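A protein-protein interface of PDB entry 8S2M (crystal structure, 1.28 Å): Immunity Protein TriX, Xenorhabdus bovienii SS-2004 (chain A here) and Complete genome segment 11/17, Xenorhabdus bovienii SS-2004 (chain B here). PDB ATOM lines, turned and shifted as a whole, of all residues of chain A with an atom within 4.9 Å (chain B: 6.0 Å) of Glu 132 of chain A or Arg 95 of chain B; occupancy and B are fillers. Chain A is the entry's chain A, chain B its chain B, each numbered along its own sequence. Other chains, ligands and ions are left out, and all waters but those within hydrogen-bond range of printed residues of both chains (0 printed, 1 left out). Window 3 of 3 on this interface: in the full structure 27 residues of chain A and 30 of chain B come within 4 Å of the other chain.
Printed residues of chain B within 4 Å of Glu 132 of chain A: Arg 95. Printed residues of chain A within 4 Å of Arg 95 of chain B: Phe 131, Glu 132 and Leu 134. Of the printed residues of chain A, Phe 98 of chain B touches Trp 130. Printed residues of chain B within 4 Å of Trp 130 of chain A: Pro 97 (3.6 Å) and Phe 98 (3.5 Å). Ala 94 of chain B touches none of the printed residues of chain A. The nearest printed residue of chain A that does not touch Arg 95 of chain B is Ser 133 of chain A (5.5 Å). The nearest printed residue of chain B that does not touch Trp 130 of chain A is Ser 96 of chain B (6.4 Å).
The guanidinium group (NH2) of Arg 95 of chain B lies within salt-bridge range of the side-chain carboxylate (OE2) of Glu 132 of chain A, 3.1 Å away. O of Phe 131 of chain A lies within hydrogen-bond range of NH2 of Arg 95 of chain B.
Of the 8 printed residues of chain B, 4 touch a printed residue of chain A. Printed residues of chain B that touch a printed residue of chain A: Tyr 40, Arg 95, Pro 97 and Phe 98. Of the 7 printed residues of chain A, 4 touch a printed residue of chain B.
O of Trp 130 of chain A lies within hydrogen-bond range of OG of Ser 133 of chain A.
Among the printed residues, pairs that only touch across the chains: Trp 130 of chain A with Phe 98 of chain B (3.5 Å), Trp 130 of chain A with Pro 97 of chain B (3.6 Å), Leu 134 of chain A with Pro 97 of chain B (3.6 Å), Leu 134 of chain A with Arg 95 of chain B (3.8 Å), Phe 131 of chain A with Pro 97 of chain B (3.8 Å) and Phe 131 of chain A with Tyr 40 of chain B (3.9 Å).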
ATOM      1  N   SER A 128       6.237   7.518 -13.119  1.00  0.00           N
ATOM      2  CA  SER A 128       5.408   7.737 -11.937  1.00  0.00           C
ATOM      3  C   SER A 128       5.348   9.214 -11.572  1.00  0.00           C
ATOM      4  O   SER A 128       4.285   9.728 -11.199  1.00  0.00           O
ATOM      5  CB  SER A 128       5.942   6.906 -10.777  1.00  0.00           C
ATOM      6  OG  SER A 128       5.524   5.557 -10.913  1.00  0.00           O
ATOM      7  N   GLN A 129       6.488   9.908 -11.653  1.00  0.00           N
ATOM      8  CA  GLN A 129       6.491  11.336 -11.362  1.00  0.00           C
ATOM      9  C   GLN A 129       5.690  12.105 -12.414  1.00  0.00           C
ATOM     10  O   GLN A 129       4.974  13.064 -12.086  1.00  0.00           O
ATOM     11  CB  GLN A 129       7.944  11.805 -11.200  1.00  0.00           C
ATOM     12  CG  GLN A 129       8.607  11.171  -9.953  1.00  0.00           C
ATOM     13  CD  GLN A 129      10.029  11.626  -9.669  1.00  0.00           C
ATOM     14  OE1 GLN A 129      10.887  11.658 -10.556  1.00  0.00           O
ATOM     15  NE2 GLN A 129      10.305  11.911  -8.399  1.00  0.00           N
ATOM     16  N   TRP A 130       5.747  11.659 -13.672  1.00  0.00           N
ATOM     17  CA  TRP A 130       4.942  12.271 -14.728  1.00  0.00           C
ATOM     18  C   TRP A 130       3.454  12.087 -14.464  1.00  0.00           C
ATOM     19  O   TRP A 130       2.665  13.032 -14.608  1.00  0.00           O
ATOM     20  CB  TRP A 130       5.314  11.680 -16.090  1.00  0.00           C
ATOM     21  CG  TRP A 130       4.382  12.139 -17.176  1.00  0.00           C
ATOM     22  CD1 TRP A 130       4.391  13.356 -17.781  1.00  0.00           C
ATOM     23  CD2 TRP A 130       3.294  11.400 -17.764  1.00  0.00           C
ATOM     24  NE1 TRP A 130       3.374  13.434 -18.700  1.00  0.00           N
ATOM     25  CE2 TRP A 130       2.684  12.246 -18.719  1.00  0.00           C
ATOM     26  CE3 TRP A 130       2.766  10.118 -17.564  1.00  0.00           C
ATOM     27  CZ2 TRP A 130       1.577  11.835 -19.491  1.00  0.00           C
ATOM     28  CZ3 TRP A 130       1.673   9.709 -18.322  1.00  0.00           C
ATOM     29  CH2 TRP A 130       1.093  10.567 -19.281  1.00  0.00           C
ATOM     30  N   PHE A 131       3.042  10.864 -14.118  1.00  0.00           N
ATOM     31  CA  PHE A 131       1.630  10.611 -13.857  1.00  0.00           C
ATOM     32  C   PHE A 131       1.127  11.488 -12.719  1.00  0.00           C
ATOM     33  O   PHE A 131       0.008  12.018 -12.774  1.00  0.00           O
ATOM     34  CB  PHE A 131       1.449   9.128 -13.538  1.00  0.00           C
ATOM     35  CG  PHE A 131       0.022   8.679 -13.440  1.00  0.00           C
ATOM     36  CD1 PHE A 131      -0.730   8.425 -14.583  1.00  0.00           C
ATOM     37  CD2 PHE A 131      -0.556   8.466 -12.204  1.00  0.00           C
ATOM     38  CE1 PHE A 131      -2.045   7.984 -14.476  1.00  0.00           C
ATOM     39  CE2 PHE A 131      -1.864   8.034 -12.091  1.00  0.00           C
ATOM     40  CZ  PHE A 131      -2.612   7.788 -13.226  1.00  0.00           C
ATOM     41  N   GLU A 132       1.961  11.694 -11.695  1.00  0.00           N
ATOM     42  CA  GLU A 132       1.571  12.540 -10.578  1.00  0.00           C
ATOM     43  C   GLU A 132       1.570  14.014 -10.958  1.00  0.00           C
ATOM     44  O   GLU A 132       0.896  14.811 -10.294  1.00  0.00           O
ATOM     45  CB  GLU A 132       2.519  12.293  -9.403  1.00  0.00           C
ATOM     46  CG  GLU A 132       2.248  10.993  -8.658  1.00  0.00           C
ATOM     47  CD  GLU A 132       0.782  10.774  -8.349  1.00  0.00           C
ATOM     48  OE1 GLU A 132       0.155  11.686  -7.762  1.00  0.00           O
ATOM     49  OE2 GLU A 132       0.254   9.698  -8.719  1.00  0.00           O
ATOM     50  N   SER A 133       2.315  14.396 -12.001  1.00  0.00           N
ATOM     51  CA  SER A 133       2.378  15.791 -12.428  1.00  0.00           C
ATOM     52  C   SER A 133       1.096  16.268 -13.083  1.00  0.00           C
ATOM     53  O   SER A 133       0.946  17.481 -13.277  1.00  0.00           O
ATOM     54  CB  SER A 133       3.557  16.020 -13.380  1.00  0.00           C
ATOM     55  OG  SER A 133       3.245  15.627 -14.710  1.00  0.00           O
ATOM     56  N   LEU A 134       0.175  15.362 -13.412  1.00  0.00           N
ATOM     57  CA  LEU A 134      -1.091  15.739 -14.029  1.00  0.00           C
ATOM     58  C   LEU A 134      -2.121  16.134 -12.978  1.00  0.00           C
ATOM     59  O   LEU A 134      -3.252  16.476 -13.323  1.00  0.00           O
ATOM     60  CB  LEU A 134      -1.637  14.604 -14.910  1.00  0.00           C
ATOM     61  CG  LEU A 134      -0.646  13.990 -15.908  1.00  0.00           C
ATOM     62  CD1 LEU A 134      -1.258  12.835 -16.678  1.00  0.00           C
ATOM     63  CD2 LEU A 134      -0.095  15.045 -16.861  1.00  0.00           C
ATOM     64  N   TYR B  40      -7.247   3.609 -11.649  1.00  0.00           N
ATOM     65  CA  TYR B  40      -6.070   4.468 -11.542  1.00  0.00           C
ATOM     66  C   TYR B  40      -4.806   3.695 -11.891  1.00  0.00           C
ATOM     67  O   TYR B  40      -3.971   4.166 -12.672  1.00  0.00           O
ATOM     68  CB  TYR B  40      -5.965   5.066 -10.137  1.00  0.00           C
ATOM     69  CG  TYR B  40      -6.817   6.292  -9.924  1.00  0.00           C
ATOM     70  CD1 TYR B  40      -8.130   6.179  -9.486  1.00  0.00           C
ATOM     71  CD2 TYR B  40      -6.315   7.563 -10.166  1.00  0.00           C
ATOM     72  CE1 TYR B  40      -8.918   7.299  -9.287  1.00  0.00           C
ATOM     73  CE2 TYR B  40      -7.098   8.686  -9.968  1.00  0.00           C
ATOM     74  CZ  TYR B  40      -8.394   8.549  -9.532  1.00  0.00           C
ATOM     75  OH  TYR B  40      -9.167   9.665  -9.341  1.00  0.00           O
ATOM     76  N   LEU B  92     -11.583   9.696 -14.470  1.00  0.00           N
ATOM     77  CA  LEU B  92     -10.335  10.244 -13.957  1.00  0.00           C
ATOM     78  C   LEU B  92     -10.246  11.759 -14.059  1.00  0.00           C
ATOM     79  O   LEU B  92      -9.412  12.359 -13.373  1.00  0.00           O
ATOM     80  CB  LEU B  92      -9.148   9.628 -14.704  1.00  0.00           C
ATOM     81  CG  LEU B  92      -8.980   8.116 -14.522  1.00  0.00           C
ATOM     82  CD1 LEU B  92      -7.669   7.664 -15.142  1.00  0.00           C
ATOM     83  CD2 LEU B  92      -9.047   7.724 -13.060  1.00  0.00           C
ATOM     84  N   GLY B  93     -11.072  12.391 -14.897  1.00  0.00           N
ATOM     85  CA  GLY B  93     -11.016  13.838 -15.002  1.00  0.00           C
ATOM     86  C   GLY B  93      -9.744  14.321 -15.683  1.00  0.00           C
ATOM     87  O   GLY B  93      -9.189  13.673 -16.575  1.00  0.00           O
ATOM     88  N   ALA B  94      -9.278  15.493 -15.243  1.00  0.00           N
ATOM     89  CA  ALA B  94      -8.082  16.109 -15.814  1.00  0.00           C
ATOM     90  C   ALA B  94      -6.833  15.259 -15.615  1.00  0.00           C
ATOM     91  O   ALA B  94      -5.828  15.481 -16.299  1.00  0.00           O
ATOM     92  CB  ALA B  94      -7.874  17.490 -15.193  1.00  0.00           C
ATOM     93  N   ARG B  95      -6.874  14.301 -14.693  1.00  0.00           N
ATOM     94  CA  ARG B  95      -5.790  13.356 -14.448  1.00  0.00           C
ATOM     95  C   ARG B  95      -5.649  12.278 -15.520  1.00  0.00           C
ATOM     96  O   ARG B  95      -4.631  11.574 -15.536  1.00  0.00           O
ATOM     97  CB  ARG B  95      -5.958  12.801 -13.030  1.00  0.00           C
ATOM     98  CG  ARG B  95      -5.767  11.327 -12.811  1.00  0.00           C
ATOM     99  CD  ARG B  95      -5.319  11.105 -11.396  1.00  0.00           C
ATOM    100  NE  ARG B  95      -3.896  11.382 -11.275  1.00  0.00           N
ATOM    101  CZ  ARG B  95      -3.200  11.271 -10.154  1.00  0.00           C
ATOM    102  NH1 ARG B  95      -3.795  11.139  -8.977  1.00  0.00           N
ATOM    103  NH2 ARG B  95      -1.872  11.305 -10.214  1.00  0.00           N
ATOM    104  N   SER B  96      -6.609  12.148 -16.420  1.00  0.00           N
ATOM    105  CA  SER B  96      -6.530  11.138 -17.468  1.00  0.00           C
ATOM    106  C   SER B  96      -5.258  11.299 -18.297  1.00  0.00           C
ATOM    107  O   SER B  96      -5.085  12.332 -18.965  1.00  0.00           O
ATOM    108  CB  SER B  96      -7.756  11.264 -18.360  1.00  0.00           C
ATOM    109  OG  SER B  96      -7.884  10.093 -19.145  1.00  0.00           O
ATOM    110  N   PRO B  97      -4.354  10.319 -18.289  1.00  0.00           N
ATOM    111  CA  PRO B  97      -3.016  10.563 -18.842  1.00  0.00           C
ATOM    112  C   PRO B  97      -2.952  10.652 -20.350  1.00  0.00           C
ATOM    113  O   PRO B  97      -2.007  11.268 -20.863  1.00  0.00           O
ATOM    114  CB  PRO B  97      -2.183   9.399 -18.285  1.00  0.00           C
ATOM    115  CG  PRO B  97      -3.176   8.318 -18.080  1.00  0.00           C
ATOM    116  CD  PRO B  97      -4.440   9.007 -17.623  1.00  0.00           C
ATOM    117  N   PHE B  98      -3.877  10.025 -21.068  1.00  0.00           N
ATOM    118  CA  PHE B  98      -3.896  10.017 -22.527  1.00  0.00           C
ATOM    119  C   PHE B  98      -5.307  10.287 -23.011  1.00  0.00           C
ATOM    120  O   PHE B  98      -5.888   9.531 -23.794  1.00  0.00           O
ATOM    121  CB  PHE B  98      -3.309   8.706 -23.054  1.00  0.00           C
ATOM    122  CG  PHE B  98      -1.916   8.439 -22.552  1.00  0.00           C
ATOM    123  CD1 PHE B  98      -0.810   9.017 -23.174  1.00  0.00           C
ATOM    124  CD2 PHE B  98      -1.716   7.663 -21.422  1.00  0.00           C
ATOM    125  CE1 PHE B  98       0.468   8.788 -22.701  1.00  0.00           C
ATOM    126  CE2 PHE B  98      -0.442   7.429 -20.947  1.00  0.00           C
ATOM    127  CZ  PHE B  98       0.651   7.987 -21.579  1.00  0.00           C
